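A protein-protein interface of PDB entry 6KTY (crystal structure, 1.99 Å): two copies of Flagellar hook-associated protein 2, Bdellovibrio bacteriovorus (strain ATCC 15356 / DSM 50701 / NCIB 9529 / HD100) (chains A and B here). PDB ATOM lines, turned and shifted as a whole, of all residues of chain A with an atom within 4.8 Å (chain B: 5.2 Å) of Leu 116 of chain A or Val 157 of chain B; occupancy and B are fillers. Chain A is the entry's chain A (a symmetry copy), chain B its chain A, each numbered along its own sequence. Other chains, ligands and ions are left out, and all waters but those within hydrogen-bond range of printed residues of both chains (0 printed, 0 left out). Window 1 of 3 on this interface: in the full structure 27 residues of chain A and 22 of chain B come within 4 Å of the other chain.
O of Leu 172 of chain B sits at hydrogen-bond distance from NE2 of Gln 101 of chain A (2.9 Å).
Among the printed residues, merely in contact across the chains: Ala 45 of chain A with Phe 160 of chain B (3.5 Å), Ala 46 of chain A with Phe 160 of chain B (3.7 Å), Met 47 of chain A with Val 157 of chain B (3.99 Å), Met 47 of chain A with Phe 160 of chain B (3.5 Å), Met 47 of chain A with Ile 162 of chain B (3.9 Å), Leu 116 of chain A with Val 157 of chain B (3.9 Å), Leu 116 of chain A with Phe 160 of chain B (3.6 Å) and Ser 118 of chain A with Asp 158 of chain B (3.5 Å).
Of the printed residues of chain B, Met 47 of chain A touches Val 157, Phe 160 and Ile 162.
Of the printed residues of chain B, Gln 101 of chain A touches Leu 172 (2.9 Å).
Val 103 of chain A touches none of the printed residues of chain B.
Leu 115 of chain A touches none of the printed residues of chain B.
Of chain B, only Val 157 and Phe 160 come within 4 Å of Leu 116 of chain A.
Of the printed residues of chain B, Ser 118 of chain A touches Asp 158.
Printed residues of chain A within 4 Å of Val 157 of chain B: Met 47 (3.99 Å) and Leu 116 (3.9 Å).
Printed residues of chain A within 4 Å of Asp 158 of chain B: Ser 118.
Along chain B the printed residues that touch a printed residue of chain A span positions 157 to 172.
Of the 12 printed residues of chain A, 6 touch a printed residue of chain B.
Hydrophobic or aromatic side chains of chain A within 4 Å of the printed part of chain B: Ala 45, Met 47 and Leu 116.
Among the printed residues, 9 pairs touch across the chains.
Among the printed residues, no Asp or Glu carboxylate lies within 4 Å of a Lys or Arg side-chain nitrogen of the other chain.
The backbone carbonyl oxygen (O) of Gln 101 of chain A is in hydrogen-bond range of the backbone NH (N) of Leu 116 of chain A (2.8 Å).
The backbone carbonyl oxygen (O) of Val 117 of chain A is in hydrogen-bond range of the backbone NH (N) of Ala 46 of chain A.
The side-chain amide oxygen (OE1) of Gln 101 of chain A lies within hydrogen-bond range of the side-chain amino group (NZ) of Lys 99 of chain A (2.9 Å).
The backbone carbonyl oxygen (O) of Ala 34 of chain B sits at hydrogen-bond distance from the backbone NH (N) of Asp 158 of chain B, 3.0 Å away.
N of Ile 162 of chain B sits at hydrogen-bond distance from O of Val 155 of chain B, 2.8 Å away.
The backbone carbonyl oxygen (O) of Ser 118 of chain A sits at hydrogen-bond distance from the backbone NH (N) of Lys 99 of chain A (2.9 Å).
No position is printed for both chains.
Of the 9 pairs that touch across the chains among the printed residues, none has its exchanged pair printed and touching as well.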
ATOM      1  N   ALA A  45       5.068  -0.450  -1.984  1.00  0.00           N
ATOM      2  CA  ALA A  45       4.805   0.323  -0.767  1.00  0.00           C
ATOM      3  C   ALA A  45       5.951   0.339   0.192  1.00  0.00           C
ATOM      4  O   ALA A  45       6.850  -0.515   0.117  1.00  0.00           O
ATOM      5  CB  ALA A  45       3.500  -0.200  -0.057  1.00  0.00           C
ATOM      6  N   ALA A  46       5.954   1.313   1.105  1.00  0.00           N
ATOM      7  CA  ALA A  46       7.019   1.370   2.140  1.00  0.00           C
ATOM      8  C   ALA A  46       6.407   1.904   3.429  1.00  0.00           C
ATOM      9  O   ALA A  46       5.395   2.672   3.412  1.00  0.00           O
ATOM     10  CB  ALA A  46       8.270   2.243   1.667  1.00  0.00           C
ATOM     11  N   MET A  47       6.926   1.451   4.546  1.00  0.00           N
ATOM     12  CA  MET A  47       6.352   1.881   5.831  1.00  0.00           C
ATOM     13  C   MET A  47       7.449   2.395   6.703  1.00  0.00           C
ATOM     14  O   MET A  47       8.500   1.743   6.813  1.00  0.00           O
ATOM     15  CB  MET A  47       5.608   0.733   6.545  1.00  0.00           C
ATOM     16  CG  MET A  47       4.739   1.205   7.733  1.00  0.00           C
ATOM     17  SD  MET A  47       3.728  -0.060   8.473  1.00  0.00           S
ATOM     18  CE  MET A  47       2.383  -0.112   7.310  1.00  0.00           C
ATOM     19  N   LYS A  99       0.160   7.426  -2.528  1.00  0.00           N
ATOM     20  CA  LYS A  99      -0.880   7.730  -1.526  1.00  0.00           C
ATOM     21  C   LYS A  99      -0.256   7.432  -0.170  1.00  0.00           C
ATOM     22  O   LYS A  99       0.323   6.366   0.019  1.00  0.00           O
ATOM     23  CB  LYS A  99      -2.130   6.871  -1.763  1.00  0.00           C
ATOM     24  CG  LYS A  99      -3.142   6.794  -0.589  1.00  0.00           C
ATOM     25  CD  LYS A  99      -4.136   5.618  -0.804  1.00  0.00           C
ATOM     26  CE  LYS A  99      -4.339   4.776   0.444  1.00  0.00           C
ATOM     27  NZ  LYS A  99      -3.055   4.185   0.983  1.00  0.00           N
ATOM     28  N   ALA A 100      -0.311   8.396   0.740  1.00  0.00           N
ATOM     29  CA  ALA A 100       0.316   8.262   2.032  1.00  0.00           C
ATOM     30  C   ALA A 100      -0.792   8.235   3.071  1.00  0.00           C
ATOM     31  O   ALA A 100      -1.807   8.895   2.922  1.00  0.00           O
ATOM     32  CB  ALA A 100       1.247   9.437   2.286  1.00  0.00           C
ATOM     33  N   GLN A 101      -0.585   7.475   4.127  1.00  0.00           N
ATOM     34  CA  GLN A 101      -1.432   7.611   5.307  1.00  0.00           C
ATOM     35  C   GLN A 101      -0.637   7.295   6.545  1.00  0.00           C
ATOM     36  O   GLN A 101       0.435   6.640   6.485  1.00  0.00           O
ATOM     37  CB  GLN A 101      -2.682   6.731   5.174  1.00  0.00           C
ATOM     38  CG  GLN A 101      -2.371   5.231   5.102  1.00  0.00           C
ATOM     39  CD  GLN A 101      -3.645   4.386   4.787  1.00  0.00           C
ATOM     40  OE1 GLN A 101      -4.197   4.444   3.683  1.00  0.00           O
ATOM     41  NE2 GLN A 101      -4.088   3.615   5.755  1.00  0.00           N
ATOM     42  N   VAL A 103      -0.541   5.183   9.986  1.00  0.00           N
ATOM     43  CA  VAL A 103      -1.200   4.081  10.652  1.00  0.00           C
ATOM     44  C   VAL A 103      -0.635   3.979  12.071  1.00  0.00           C
ATOM     45  O   VAL A 103       0.430   4.543  12.363  1.00  0.00           O
ATOM     46  CB  VAL A 103      -1.050   2.753   9.849  1.00  0.00           C
ATOM     47  CG1 VAL A 103      -1.645   2.882   8.435  1.00  0.00           C
ATOM     48  CG2 VAL A 103       0.403   2.291   9.809  1.00  0.00           C
ATOM     49  N   LYS A 114       3.113   5.206  12.288  1.00  0.00           N
ATOM     50  CA  LYS A 114       3.949   4.975  11.108  1.00  0.00           C
ATOM     51  C   LYS A 114       3.389   5.547   9.841  1.00  0.00           C
ATOM     52  O   LYS A 114       2.155   5.580   9.647  1.00  0.00           O
ATOM     53  CB  LYS A 114       4.201   3.493  10.949  1.00  0.00           C
ATOM     54  CG  LYS A 114       5.067   2.943  12.049  1.00  0.00           C
ATOM     55  CD  LYS A 114       5.127   1.463  11.961  1.00  0.00           C
ATOM     56  CE  LYS A 114       5.964   0.905  13.114  1.00  0.00           C
ATOM     57  NZ  LYS A 114       6.166  -0.556  13.043  1.00  0.00           N
ATOM     58  N   LEU A 115       4.283   6.056   8.996  1.00  0.00           N
ATOM     59  CA  LEU A 115       3.890   6.559   7.686  1.00  0.00           C
ATOM     60  C   LEU A 115       3.922   5.380   6.727  1.00  0.00           C
ATOM     61  O   LEU A 115       4.914   4.647   6.676  1.00  0.00           O
ATOM     62  CB  LEU A 115       4.830   7.667   7.209  1.00  0.00           C
ATOM     63  CG  LEU A 115       4.530   8.279   5.832  1.00  0.00           C
ATOM     64  CD1 LEU A 115       3.298   9.197   5.896  1.00  0.00           C
ATOM     65  CD2 LEU A 115       5.750   9.050   5.348  1.00  0.00           C
ATOM     66  N   LEU A 116       2.805   5.165   6.039  1.00  0.00           N
ATOM     67  CA  LEU A 116       2.697   4.156   4.987  1.00  0.00           C
ATOM     68  C   LEU A 116       2.562   4.875   3.654  1.00  0.00           C
ATOM     69  O   LEU A 116       1.645   5.696   3.475  1.00  0.00           O
ATOM     70  CB  LEU A 116       1.462   3.272   5.232  1.00  0.00           C
ATOM     71  CG  LEU A 116       0.985   2.348   4.076  1.00  0.00           C
ATOM     72  CD1 LEU A 116       2.018   1.250   3.839  1.00  0.00           C
ATOM     73  CD2 LEU A 116      -0.390   1.703   4.382  1.00  0.00           C
ATOM     74  N   VAL A 117       3.434   4.575   2.708  1.00  0.00           N
ATOM     75  CA  VAL A 117       3.349   5.224   1.390  1.00  0.00           C
ATOM     76  C   VAL A 117       3.192   4.083   0.348  1.00  0.00           C
ATOM     77  O   VAL A 117       4.012   3.175   0.304  1.00  0.00           O
ATOM     78  CB  VAL A 117       4.595   6.057   1.127  1.00  0.00           C
ATOM     79  CG1 VAL A 117       4.565   6.703  -0.247  1.00  0.00           C
ATOM     80  CG2 VAL A 117       4.800   7.133   2.240  1.00  0.00           C
ATOM     81  N   SER A 118       2.163   4.141  -0.482  1.00  0.00           N
ATOM     82  CA  SER A 118       1.927   3.084  -1.458  1.00  0.00           C
ATOM     83  C   SER A 118       1.690   3.655  -2.857  1.00  0.00           C
ATOM     84  O   SER A 118       1.141   4.747  -2.996  1.00  0.00           O
ATOM     85  CB  SER A 118       0.779   2.230  -0.979  1.00  0.00           C
ATOM     86  OG  SER A 118      -0.433   2.956  -1.144  1.00  0.00           O
ATOM     87  N   ALA B  34      -5.965  -3.039   0.635  1.00  0.00           N
ATOM     88  CA  ALA B  34      -5.669  -4.469   0.728  1.00  0.00           C
ATOM     89  C   ALA B  34      -5.454  -4.804   2.193  1.00  0.00           C
ATOM     90  O   ALA B  34      -4.467  -4.346   2.789  1.00  0.00           O
ATOM     91  CB  ALA B  34      -4.446  -4.797  -0.064  1.00  0.00           C
ATOM     92  N   ILE B  35      -6.381  -5.585   2.765  1.00  0.00           N
ATOM     93  CA  ILE B  35      -6.348  -5.920   4.192  1.00  0.00           C
ATOM     94  C   ILE B  35      -6.474  -7.405   4.377  1.00  0.00           C
ATOM     95  O   ILE B  35      -7.370  -8.034   3.797  1.00  0.00           O
ATOM     96  CB  ILE B  35      -7.498  -5.257   4.990  1.00  0.00           C
ATOM     97  CG1 ILE B  35      -7.433  -3.745   4.900  1.00  0.00           C
ATOM     98  CG2 ILE B  35      -7.412  -5.616   6.475  1.00  0.00           C
ATOM     99  CD1 ILE B  35      -6.095  -3.143   5.309  1.00  0.00           C
ATOM    100  N   VAL B 155      -2.893  -7.523  11.608  1.00  0.00           N
ATOM    101  CA  VAL B 155      -3.438  -7.313  10.300  1.00  0.00           C
ATOM    102  C   VAL B 155      -2.381  -6.824   9.343  1.00  0.00           C
ATOM    103  O   VAL B 155      -1.453  -6.128   9.735  1.00  0.00           O
ATOM    104  CB  VAL B 155      -4.587  -6.312  10.341  1.00  0.00           C
ATOM    105  CG1 VAL B 155      -5.600  -6.780  11.415  1.00  0.00           C
ATOM    106  CG2 VAL B 155      -4.080  -4.925  10.640  1.00  0.00           C
ATOM    107  N   LYS B 156      -2.542  -7.144   8.080  1.00  0.00           N
ATOM    108  CA  LYS B 156      -1.657  -6.608   7.081  1.00  0.00           C
ATOM    109  C   LYS B 156      -2.372  -5.566   6.239  1.00  0.00           C
ATOM    110  O   LYS B 156      -3.468  -5.810   5.724  1.00  0.00           O
ATOM    111  CB  LYS B 156      -1.102  -7.707   6.191  1.00  0.00           C
ATOM    112  CG  LYS B 156      -0.228  -8.741   6.932  1.00  0.00           C
ATOM    113  CD  LYS B 156       0.370  -9.752   5.933  1.00  0.00           C
ATOM    114  CE  LYS B 156       1.408 -10.662   6.644  1.00  0.00           C
ATOM    115  NZ  LYS B 156       1.931 -11.767   5.803  1.00  0.00           N
ATOM    116  N   VAL B 157      -1.719  -4.423   6.081  1.00  0.00           N
ATOM    117  CA  VAL B 157      -2.227  -3.367   5.233  1.00  0.00           C
ATOM    118  C   VAL B 157      -1.195  -3.185   4.117  1.00  0.00           C
ATOM    119  O   VAL B 157      -0.003  -2.990   4.377  1.00  0.00           O
ATOM    120  CB  VAL B 157      -2.527  -2.083   6.026  1.00  0.00           C
ATOM    121  CG1 VAL B 157      -1.292  -1.575   6.761  1.00  0.00           C
ATOM    122  CG2 VAL B 157      -3.138  -1.022   5.113  1.00  0.00           C
ATOM    123  N   ASP B 158      -1.666  -3.327   2.879  1.00  0.00           N
ATOM    124  CA  ASP B 158      -0.797  -3.402   1.694  1.00  0.00           C
ATOM    125  C   ASP B 158       0.438  -4.302   1.932  1.00  0.00           C
ATOM    126  O   ASP B 158       1.551  -3.972   1.524  1.00  0.00           O
ATOM    127  CB  ASP B 158      -0.374  -1.997   1.275  1.00  0.00           C
ATOM    128  CG  ASP B 158      -1.544  -1.158   0.715  1.00  0.00           C
ATOM    129  OD1 ASP B 158      -2.585  -1.725   0.277  1.00  0.00           O
ATOM    130  OD2 ASP B 158      -1.402   0.078   0.699  1.00  0.00           O
ATOM    131  N   GLY B 159       0.218  -5.420   2.616  1.00  0.00           N
ATOM    132  CA  GLY B 159       1.261  -6.405   2.880  1.00  0.00           C
ATOM    133  C   GLY B 159       2.102  -6.207   4.114  1.00  0.00           C
ATOM    134  O   GLY B 159       2.953  -7.047   4.380  1.00  0.00           O
ATOM    135  N   PHE B 160       1.903  -5.106   4.865  1.00  0.00           N
ATOM    136  CA  PHE B 160       2.667  -4.857   6.080  1.00  0.00           C
ATOM    137  C   PHE B 160       1.867  -5.256   7.300  1.00  0.00           C
ATOM    138  O   PHE B 160       0.753  -4.749   7.506  1.00  0.00           O
ATOM    139  CB  PHE B 160       3.028  -3.388   6.228  1.00  0.00           C
ATOM    140  CG  PHE B 160       3.872  -2.864   5.132  1.00  0.00           C
ATOM    141  CD1 PHE B 160       5.238  -3.131   5.095  1.00  0.00           C
ATOM    142  CD2 PHE B 160       3.321  -2.100   4.140  1.00  0.00           C
ATOM    143  CE1 PHE B 160       6.025  -2.653   4.086  1.00  0.00           C
ATOM    144  CE2 PHE B 160       4.134  -1.588   3.122  1.00  0.00           C
ATOM    145  CZ  PHE B 160       5.489  -1.867   3.112  1.00  0.00           C
ATOM    146  N   GLU B 161       2.451  -6.119   8.140  1.00  0.00           N
ATOM    147  CA  GLU B 161       1.759  -6.595   9.333  1.00  0.00           C
ATOM    148  C   GLU B 161       1.910  -5.555  10.448  1.00  0.00           C
ATOM    149  O   GLU B 161       3.006  -5.172  10.776  1.00  0.00           O
ATOM    150  CB  GLU B 161       2.295  -7.971   9.801  1.00  0.00           C
ATOM    151  CG  GLU B 161       1.594  -8.453  11.048  1.00  0.00           C
ATOM    152  CD  GLU B 161       1.986  -9.851  11.462  1.00  0.00           C
ATOM    153  OE1 GLU B 161       2.591  -9.978  12.541  1.00  0.00           O
ATOM    154  OE2 GLU B 161       1.699 -10.799  10.702  1.00  0.00           O
ATOM    155  N   ILE B 162       0.788  -5.058  10.957  1.00  0.00           N
ATOM    156  CA  ILE B 162       0.776  -4.166  12.094  1.00  0.00           C
ATOM    157  C   ILE B 162      -0.141  -4.748  13.162  1.00  0.00           C
ATOM    158  O   ILE B 162      -0.936  -5.673  12.892  1.00  0.00           O
ATOM    159  CB  ILE B 162       0.336  -2.746  11.706  1.00  0.00           C
ATOM    160  CG1 ILE B 162      -1.113  -2.728  11.209  1.00  0.00           C
ATOM    161  CG2 ILE B 162       1.290  -2.169  10.653  1.00  0.00           C
ATOM    162  CD1 ILE B 162      -1.623  -1.363  10.936  1.00  0.00           C
ATOM    163  N   LEU B 172      -7.058   2.315   9.191  1.00  0.00           N
ATOM    164  CA  LEU B 172      -6.609   1.557   8.011  1.00  0.00           C
ATOM    165  C   LEU B 172      -7.217   2.023   6.700  1.00  0.00           C
ATOM    166  O   LEU B 172      -6.542   2.053   5.667  1.00  0.00           O
ATOM    167  CB  LEU B 172      -6.879   0.083   8.225  1.00  0.00           C
ATOM    168  CG  LEU B 172      -5.984  -0.445   9.333  1.00  0.00           C
ATOM    169  CD1 LEU B 172      -5.997  -1.928   9.396  1.00  0.00           C
ATOM    170  CD2 LEU B 172      -4.557   0.101   9.064  1.00  0.00           C
